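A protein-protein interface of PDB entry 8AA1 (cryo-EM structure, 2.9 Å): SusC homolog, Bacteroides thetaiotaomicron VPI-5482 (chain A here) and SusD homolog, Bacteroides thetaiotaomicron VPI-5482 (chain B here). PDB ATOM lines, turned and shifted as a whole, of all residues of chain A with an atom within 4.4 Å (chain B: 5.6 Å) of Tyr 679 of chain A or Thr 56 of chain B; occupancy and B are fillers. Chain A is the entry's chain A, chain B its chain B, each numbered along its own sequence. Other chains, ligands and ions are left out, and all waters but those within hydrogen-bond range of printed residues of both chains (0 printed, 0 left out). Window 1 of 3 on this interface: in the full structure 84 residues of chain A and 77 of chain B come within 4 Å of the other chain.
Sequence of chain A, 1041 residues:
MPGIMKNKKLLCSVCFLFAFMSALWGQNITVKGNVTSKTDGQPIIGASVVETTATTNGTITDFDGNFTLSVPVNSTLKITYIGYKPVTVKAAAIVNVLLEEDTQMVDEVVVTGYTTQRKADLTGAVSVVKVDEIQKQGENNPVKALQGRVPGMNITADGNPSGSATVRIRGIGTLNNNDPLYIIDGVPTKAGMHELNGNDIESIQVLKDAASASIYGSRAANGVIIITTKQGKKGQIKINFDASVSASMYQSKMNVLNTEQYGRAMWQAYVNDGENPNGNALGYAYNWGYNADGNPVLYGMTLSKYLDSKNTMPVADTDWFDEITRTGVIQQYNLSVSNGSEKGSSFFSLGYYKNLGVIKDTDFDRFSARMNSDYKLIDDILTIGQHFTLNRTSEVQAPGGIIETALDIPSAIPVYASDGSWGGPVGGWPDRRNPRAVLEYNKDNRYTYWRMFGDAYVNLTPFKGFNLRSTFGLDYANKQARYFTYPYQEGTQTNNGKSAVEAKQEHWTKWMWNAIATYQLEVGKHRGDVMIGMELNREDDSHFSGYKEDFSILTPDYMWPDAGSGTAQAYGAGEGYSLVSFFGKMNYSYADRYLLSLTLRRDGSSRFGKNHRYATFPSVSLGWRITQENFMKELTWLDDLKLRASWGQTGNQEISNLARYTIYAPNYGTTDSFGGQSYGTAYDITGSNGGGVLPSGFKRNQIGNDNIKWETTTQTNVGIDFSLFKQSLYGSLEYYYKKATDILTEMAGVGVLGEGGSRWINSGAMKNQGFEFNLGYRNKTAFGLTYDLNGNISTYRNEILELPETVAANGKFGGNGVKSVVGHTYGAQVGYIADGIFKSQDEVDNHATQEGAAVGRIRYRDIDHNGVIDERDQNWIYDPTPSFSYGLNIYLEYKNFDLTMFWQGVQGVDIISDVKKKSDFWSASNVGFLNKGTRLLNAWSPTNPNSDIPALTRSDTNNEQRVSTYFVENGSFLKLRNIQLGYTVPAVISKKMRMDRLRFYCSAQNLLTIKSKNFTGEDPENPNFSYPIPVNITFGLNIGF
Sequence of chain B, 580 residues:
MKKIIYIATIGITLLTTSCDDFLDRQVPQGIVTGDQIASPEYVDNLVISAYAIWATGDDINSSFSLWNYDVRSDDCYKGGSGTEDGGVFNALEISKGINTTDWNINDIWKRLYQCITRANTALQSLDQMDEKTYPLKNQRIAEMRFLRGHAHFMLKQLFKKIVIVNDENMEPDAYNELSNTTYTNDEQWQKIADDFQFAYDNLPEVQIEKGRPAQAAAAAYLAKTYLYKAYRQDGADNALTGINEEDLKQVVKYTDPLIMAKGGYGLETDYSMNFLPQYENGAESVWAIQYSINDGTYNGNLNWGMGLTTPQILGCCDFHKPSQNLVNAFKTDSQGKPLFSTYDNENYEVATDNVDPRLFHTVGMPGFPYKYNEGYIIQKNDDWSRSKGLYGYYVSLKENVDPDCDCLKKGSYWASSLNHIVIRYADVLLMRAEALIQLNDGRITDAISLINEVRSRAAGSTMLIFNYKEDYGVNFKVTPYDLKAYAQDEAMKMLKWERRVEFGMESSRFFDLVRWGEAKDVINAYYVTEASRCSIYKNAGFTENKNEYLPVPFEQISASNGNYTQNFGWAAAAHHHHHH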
ATOM      1  N   ASN A 667      21.217   0.259 -23.137  1.00  0.00           N
ATOM      2  CA  ASN A 667      20.746   0.973 -21.958  1.00  0.00           C
ATOM      3  C   ASN A 667      19.409   0.411 -21.496  1.00  0.00           C
ATOM      4  O   ASN A 667      18.349   0.867 -21.937  1.00  0.00           O
ATOM      5  CB  ASN A 667      20.627   2.469 -22.249  1.00  0.00           C
ATOM      6  CG  ASN A 667      20.335   3.282 -21.005  1.00  0.00           C
ATOM      7  OD1 ASN A 667      19.188   3.628 -20.730  1.00  0.00           O
ATOM      8  ND2 ASN A 667      21.377   3.590 -20.243  1.00  0.00           N
ATOM      9  N   GLY A 676      12.156  10.950 -15.302  1.00  0.00           N
ATOM     10  CA  GLY A 676      11.786   9.811 -16.112  1.00  0.00           C
ATOM     11  C   GLY A 676      12.357   9.787 -17.512  1.00  0.00           C
ATOM     12  O   GLY A 676      12.009   8.886 -18.286  1.00  0.00           O
ATOM     13  N   GLN A 677      13.217  10.736 -17.868  1.00  0.00           N
ATOM     14  CA  GLN A 677      13.845  10.749 -19.189  1.00  0.00           C
ATOM     15  C   GLN A 677      15.099   9.880 -19.217  1.00  0.00           C
ATOM     16  O   GLN A 677      16.182  10.318 -19.602  1.00  0.00           O
ATOM     17  CB  GLN A 677      14.159  12.182 -19.602  1.00  0.00           C
ATOM     18  CG  GLN A 677      14.899  12.989 -18.550  1.00  0.00           C
ATOM     19  CD  GLN A 677      15.296  14.363 -19.047  1.00  0.00           C
ATOM     20  OE1 GLN A 677      15.173  14.665 -20.233  1.00  0.00           O
ATOM     21  NE2 GLN A 677      15.775  15.205 -18.139  1.00  0.00           N
ATOM     22  N   SER A 678      14.951   8.621 -18.804  1.00  0.00           N
ATOM     23  CA  SER A 678      16.091   7.715 -18.751  1.00  0.00           C
ATOM     24  C   SER A 678      16.523   7.238 -20.129  1.00  0.00           C
ATOM     25  O   SER A 678      17.665   6.796 -20.285  1.00  0.00           O
ATOM     26  CB  SER A 678      15.761   6.510 -17.869  1.00  0.00           C
ATOM     27  OG  SER A 678      14.651   5.795 -18.381  1.00  0.00           O
ATOM     28  N   TYR A 679      15.637   7.320 -21.125  1.00  0.00           N
ATOM     29  CA  TYR A 679      15.907   6.823 -22.475  1.00  0.00           C
ATOM     30  C   TYR A 679      16.310   5.353 -22.460  1.00  0.00           C
ATOM     31  O   TYR A 679      17.117   4.909 -23.278  1.00  0.00           O
ATOM     32  CB  TYR A 679      16.975   7.663 -23.180  1.00  0.00           C
ATOM     33  CG  TYR A 679      16.542   9.079 -23.474  1.00  0.00           C
ATOM     34  CD1 TYR A 679      15.738   9.367 -24.567  1.00  0.00           C
ATOM     35  CD2 TYR A 679      16.938  10.130 -22.658  1.00  0.00           C
ATOM     36  CE1 TYR A 679      15.338  10.660 -24.838  1.00  0.00           C
ATOM     37  CE2 TYR A 679      16.545  11.426 -22.921  1.00  0.00           C
ATOM     38  CZ  TYR A 679      15.745  11.685 -24.013  1.00  0.00           C
ATOM     39  OH  TYR A 679      15.351  12.975 -24.280  1.00  0.00           O
ATOM     40  N   GLY A 680      15.747   4.588 -21.527  1.00  0.00           N
ATOM     41  CA  GLY A 680      16.085   3.187 -21.423  1.00  0.00           C
ATOM     42  C   GLY A 680      15.512   2.370 -22.563  1.00  0.00           C
ATOM     43  O   GLY A 680      14.611   2.793 -23.287  1.00  0.00           O
ATOM     44  N   THR A 681      16.058   1.169 -22.725  1.00  0.00           N
ATOM     45  CA  THR A 681      15.635   0.246 -23.775  1.00  0.00           C
ATOM     46  C   THR A 681      15.062  -1.000 -23.109  1.00  0.00           C
ATOM     47  O   THR A 681      15.751  -2.006 -22.935  1.00  0.00           O
ATOM     48  CB  THR A 681      16.791  -0.092 -24.690  1.00  0.00           C
ATOM     49  OG1 THR A 681      17.546   1.093 -24.964  1.00  0.00           O
ATOM     50  CG2 THR A 681      16.270  -0.653 -25.987  1.00  0.00           C
ATOM     51  N   LYS A 699      20.562   1.524 -28.114  1.00  0.00           N
ATOM     52  CA  LYS A 699      20.318   2.907 -28.488  1.00  0.00           C
ATOM     53  C   LYS A 699      21.640   3.559 -28.869  1.00  0.00           C
ATOM     54  O   LYS A 699      22.706   3.161 -28.393  1.00  0.00           O
ATOM     55  CB  LYS A 699      19.644   3.696 -27.357  1.00  0.00           C
ATOM     56  CG  LYS A 699      20.570   4.078 -26.215  1.00  0.00           C
ATOM     57  CD  LYS A 699      19.870   4.999 -25.233  1.00  0.00           C
ATOM     58  CE  LYS A 699      20.846   5.579 -24.225  1.00  0.00           C
ATOM     59  NZ  LYS A 699      21.903   6.391 -24.884  1.00  0.00           N
ATOM     60  N   ALA B  52      10.533   1.172 -26.743  1.00  0.00           N
ATOM     61  CA  ALA B  52      10.941   1.653 -25.428  1.00  0.00           C
ATOM     62  C   ALA B  52      11.030   3.170 -25.386  1.00  0.00           C
ATOM     63  O   ALA B  52      10.745   3.779 -24.347  1.00  0.00           O
ATOM     64  CB  ALA B  52      12.279   1.030 -25.035  1.00  0.00           C
ATOM     65  N   ILE B  53      11.408   3.797 -26.502  1.00  0.00           N
ATOM     66  CA  ILE B  53      11.505   5.253 -26.543  1.00  0.00           C
ATOM     67  C   ILE B  53      10.143   5.891 -26.306  1.00  0.00           C
ATOM     68  O   ILE B  53      10.058   7.036 -25.849  1.00  0.00           O
ATOM     69  CB  ILE B  53      12.127   5.708 -27.879  1.00  0.00           C
ATOM     70  CG1 ILE B  53      12.552   7.174 -27.802  1.00  0.00           C
ATOM     71  CG2 ILE B  53      11.160   5.486 -29.029  1.00  0.00           C
ATOM     72  CD1 ILE B  53      13.541   7.465 -26.701  1.00  0.00           C
ATOM     73  N   TRP B  54       9.062   5.168 -26.597  1.00  0.00           N
ATOM     74  CA  TRP B  54       7.725   5.696 -26.359  1.00  0.00           C
ATOM     75  C   TRP B  54       7.298   5.583 -24.903  1.00  0.00           C
ATOM     76  O   TRP B  54       6.271   6.162 -24.531  1.00  0.00           O
ATOM     77  CB  TRP B  54       6.711   4.983 -27.253  1.00  0.00           C
ATOM     78  CG  TRP B  54       6.800   5.406 -28.682  1.00  0.00           C
ATOM     79  CD1 TRP B  54       7.302   4.683 -29.721  1.00  0.00           C
ATOM     80  CD2 TRP B  54       6.387   6.662 -29.229  1.00  0.00           C
ATOM     81  NE1 TRP B  54       7.222   5.407 -30.885  1.00  0.00           N
ATOM     82  CE2 TRP B  54       6.663   6.627 -30.609  1.00  0.00           C
ATOM     83  CE3 TRP B  54       5.807   7.813 -28.687  1.00  0.00           C
ATOM     84  CZ2 TRP B  54       6.380   7.696 -31.454  1.00  0.00           C
ATOM     85  CZ3 TRP B  54       5.526   8.873 -29.527  1.00  0.00           C
ATOM     86  CH2 TRP B  54       5.813   8.808 -30.895  1.00  0.00           C
ATOM     87  N   ALA B  55       8.053   4.861 -24.074  1.00  0.00           N
ATOM     88  CA  ALA B  55       7.752   4.745 -22.656  1.00  0.00           C
ATOM     89  C   ALA B  55       8.827   5.322 -21.750  1.00  0.00           C
ATOM     90  O   ALA B  55       8.546   5.559 -20.570  1.00  0.00           O
ATOM     91  CB  ALA B  55       7.523   3.275 -22.271  1.00  0.00           C
ATOM     92  N   THR B  56      10.038   5.555 -22.256  1.00  0.00           N
ATOM     93  CA  THR B  56      11.132   6.072 -21.450  1.00  0.00           C
ATOM     94  C   THR B  56      11.686   7.393 -21.962  1.00  0.00           C
ATOM     95  O   THR B  56      12.534   7.992 -21.289  1.00  0.00           O
ATOM     96  CB  THR B  56      12.270   5.045 -21.374  1.00  0.00           C
ATOM     97  OG1 THR B  56      12.750   4.764 -22.693  1.00  0.00           O
ATOM     98  CG2 THR B  56      11.783   3.755 -20.736  1.00  0.00           C
ATOM     99  N   GLY B  57      11.242   7.865 -23.121  1.00  0.00           N
ATOM    100  CA  GLY B  57      11.745   9.086 -23.706  1.00  0.00           C
ATOM    101  C   GLY B  57      10.974  10.344 -23.381  1.00  0.00           C
ATOM    102  O   GLY B  57      11.286  11.402 -23.937  1.00  0.00           O
ATOM    103  N   ASP B  58       9.982  10.272 -22.500  1.00  0.00           N
ATOM    104  CA  ASP B  58       9.148  11.415 -22.157  1.00  0.00           C
ATOM    105  C   ASP B  58       9.488  11.900 -20.755  1.00  0.00           C
ATOM    106  O   ASP B  58       9.639  11.092 -19.833  1.00  0.00           O
ATOM    107  CB  ASP B  58       7.663  11.057 -22.250  1.00  0.00           C
ATOM    108  CG  ASP B  58       7.300   9.850 -21.410  1.00  0.00           C
ATOM    109  OD1 ASP B  58       8.164   8.967 -21.231  1.00  0.00           O
ATOM    110  OD2 ASP B  58       6.149   9.783 -20.930  1.00  0.00           O
ATOM    111  N   PHE B  64       4.357  12.260 -24.049  1.00  0.00           N
ATOM    112  CA  PHE B  64       3.811  11.896 -25.348  1.00  0.00           C
ATOM    113  C   PHE B  64       2.289  11.926 -25.375  1.00  0.00           C
ATOM    114  O   PHE B  64       1.706  11.837 -26.459  1.00  0.00           O
ATOM    115  CB  PHE B  64       4.328  10.517 -25.754  1.00  0.00           C
ATOM    116  CG  PHE B  64       5.816  10.469 -25.938  1.00  0.00           C
ATOM    117  CD1 PHE B  64       6.499  11.569 -26.429  1.00  0.00           C
ATOM    118  CD2 PHE B  64       6.534   9.333 -25.608  1.00  0.00           C
ATOM    119  CE1 PHE B  64       7.867  11.534 -26.598  1.00  0.00           C
ATOM    120  CE2 PHE B  64       7.904   9.294 -25.774  1.00  0.00           C
ATOM    121  CZ  PHE B  64       8.571  10.395 -26.269  1.00  0.00           C
ATOM    122  N   ASP B 107      12.393  21.135 -26.613  1.00  0.00           N
ATOM    123  CA  ASP B 107      12.519  19.829 -25.977  1.00  0.00           C
ATOM    124  C   ASP B 107      11.562  18.817 -26.597  1.00  0.00           C
ATOM    125  O   ASP B 107      11.952  17.684 -26.897  1.00  0.00           O
ATOM    126  CB  ASP B 107      12.272  19.958 -24.474  1.00  0.00           C
ATOM    127  CG  ASP B 107      12.512  18.660 -23.731  1.00  0.00           C
ATOM    128  OD1 ASP B 107      13.685  18.252 -23.608  1.00  0.00           O
ATOM    129  OD2 ASP B 107      11.526  18.048 -23.268  1.00  0.00           O
ATOM    130  N   ARG B 111      12.572  15.483 -28.696  1.00  0.00           N
ATOM    131  CA  ARG B 111      12.170  14.155 -28.240  1.00  0.00           C
ATOM    132  C   ARG B 111      11.387  13.407 -29.315  1.00  0.00           C
ATOM    133  O   ARG B 111      11.624  12.211 -29.553  1.00  0.00           O
ATOM    134  CB  ARG B 111      11.348  14.267 -26.957  1.00  0.00           C
ATOM    135  CG  ARG B 111      12.152  14.735 -25.759  1.00  0.00           C
ATOM    136  CD  ARG B 111      11.319  14.733 -24.494  1.00  0.00           C
ATOM    137  NE  ARG B 111      11.982  15.453 -23.413  1.00  0.00           N
ATOM    138  CZ  ARG B 111      12.902  14.929 -22.617  1.00  0.00           C
ATOM    139  NH1 ARG B 111      13.298  13.673 -22.750  1.00  0.00           N
ATOM    140  NH2 ARG B 111      13.442  15.683 -21.664  1.00  0.00           N
ATOM    141  N   GLN B 114      13.741  12.300 -31.861  1.00  0.00           N
ATOM    142  CA  GLN B 114      14.523  11.176 -31.357  1.00  0.00           C
ATOM    143  C   GLN B 114      13.770   9.866 -31.538  1.00  0.00           C
ATOM    144  O   GLN B 114      14.352   8.856 -31.959  1.00  0.00           O
ATOM    145  CB  GLN B 114      14.864  11.389 -29.882  1.00  0.00           C
ATOM    146  CG  GLN B 114      15.985  12.377 -29.630  1.00  0.00           C
ATOM    147  CD  GLN B 114      16.090  12.772 -28.173  1.00  0.00           C
ATOM    148  OE1 GLN B 114      15.167  12.550 -27.390  1.00  0.00           O
ATOM    149  NE2 GLN B 114      17.217  13.366 -27.799  1.00  0.00           N
ATOM    150  N   ARG B 118      15.011   6.738 -33.909  1.00  0.00           N
ATOM    151  CA  ARG B 118      15.099   5.364 -33.417  1.00  0.00           C
ATOM    152  C   ARG B 118      14.305   4.417 -34.311  1.00  0.00           C
ATOM    153  O   ARG B 118      14.793   3.337 -34.687  1.00  0.00           O
ATOM    154  CB  ARG B 118      14.616   5.276 -31.971  1.00  0.00           C
ATOM    155  CG  ARG B 118      15.000   3.969 -31.299  1.00  0.00           C
ATOM    156  CD  ARG B 118      14.693   3.960 -29.812  1.00  0.00           C
ATOM    157  NE  ARG B 118      15.661   4.717 -29.026  1.00  0.00           N
ATOM    158  CZ  ARG B 118      15.744   4.668 -27.704  1.00  0.00           C
ATOM    159  NH1 ARG B 118      14.938   3.902 -26.988  1.00  0.00           N
ATOM    160  NH2 ARG B 118      16.664   5.402 -27.084  1.00  0.00           N
ATOM    161  N   ASN B 301       9.108   0.891 -15.801  1.00  0.00           N
ATOM    162  CA  ASN B 301       8.722   1.715 -16.946  1.00  0.00           C
ATOM    163  C   ASN B 301       7.358   2.347 -16.670  1.00  0.00           C
ATOM    164  O   ASN B 301       6.348   2.053 -17.312  1.00  0.00           O
ATOM    165  CB  ASN B 301       8.712   0.888 -18.223  1.00  0.00           C
ATOM    166  CG  ASN B 301      10.103   0.517 -18.688  1.00  0.00           C
ATOM    167  OD1 ASN B 301      11.066   1.244 -18.446  1.00  0.00           O
ATOM    168  ND2 ASN B 301      10.218  -0.621 -19.361  1.00  0.00           N
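NH2 of Arg 111 of chain B lies within hydrogen-bond range of OE1 of Gln 677 of chain A, 2.5 Å away. The backbone carbonyl oxygen (O) of Thr 56 of chain B lies within hydrogen-bond range of the backbone NH (N) of Tyr 679 of chain A (3.2 Å). O of Gly 680 of chain A sits at hydrogen-bond distance from OG1 of Thr 56 of chain B (2.8 Å). The guanidinium group (NH1) of Arg 111 of chain B lies within hydrogen-bond range of the side-chain hydroxyl (OH) of Tyr 679 of chain A (2.7 Å). The side-chain hydroxyl (OH) of Tyr 679 of chain A lies within hydrogen-bond range of the side-chain amide oxygen (OE1) of Gln 114 of chain B (3.1 Å). The backbone carbonyl oxygen (O) of Gly 676 of chain A sits close to the backbone carbonyl oxygen (O) of Thr 56 of chain B (3.2 Å).
The side-chain hydroxyl (OG1) of Thr 56 of chain B sits at hydrogen-bond distance from the backbone carbonyl oxygen (O) of Ala 52 of chain B (2.8 Å). The backbone carbonyl oxygen of Gly 57 of chain B is in hydrogen-bond range of the guanidinium group of Arg 111 of chain B (3.3 Å). O of Asn 667 of chain A lies within hydrogen-bond range of N of Thr 681 of chain A. The side-chain carboxylate of Asp 107 of chain B lies within salt-bridge range of the guanidinium group of Arg 111 of chain B.
Among the printed residues, pairs that only touch across the chains: Gly 680 of chain A with Ala 52 of chain B, Lys 699 of chain A with Arg 118 of chain B, Ser 678 of chain A with Thr 56 of chain B, Gly 676 of chain A with Asp 58 of chain B, Tyr 679 of chain A with Ile 53 of chain B, Thr 681 of chain A with Ala 52 of chain B, Gln 677 of chain A with Thr 56 of chain B, Tyr 679 of chain A with Arg 118 of chain B and Gly 680 of chain A with Arg 118 of chain B.
Of chain B, only Ile 53, Thr 56, Arg 111, Gln 114 and Arg 118 come within 4 Å of Tyr 679 of chain A. Of chain A, only Gly 676, Gln 677, Ser 678, Tyr 679 and Gly 680 come within 4 Å of Thr 56 of chain B. Of the printed residues of chain B, Thr 681 of chain A touches Ala 52. Printed residues of chain A within 4 Å of Ala 52 of chain B: Gly 680 and Thr 681. Phe 64 of chain B touches none of the printed residues of chain A. The nearest residue of chain B that does not touch Tyr 679 of chain A is Gly 57 of chain B (4.1 Å).
Of the 13 printed residues of chain B, 7 touch a printed residue of chain A. Printed residues of chain B that touch a printed residue of chain A: Ala 52, Ile 53, Thr 56, Asp 58, Arg 111, Gln 114 and Arg 118. Hydrophobic or aromatic side chains of chain B that line the printed part of chain A: Ala 52 and Ile 53. Along chain B the printed residues that touch a printed residue of chain A span positions 52 to 118. Along chain A the printed residues that touch a printed residue of chain B span positions 676 to 699. Among the printed residues, 15 pairs touch across the chains.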
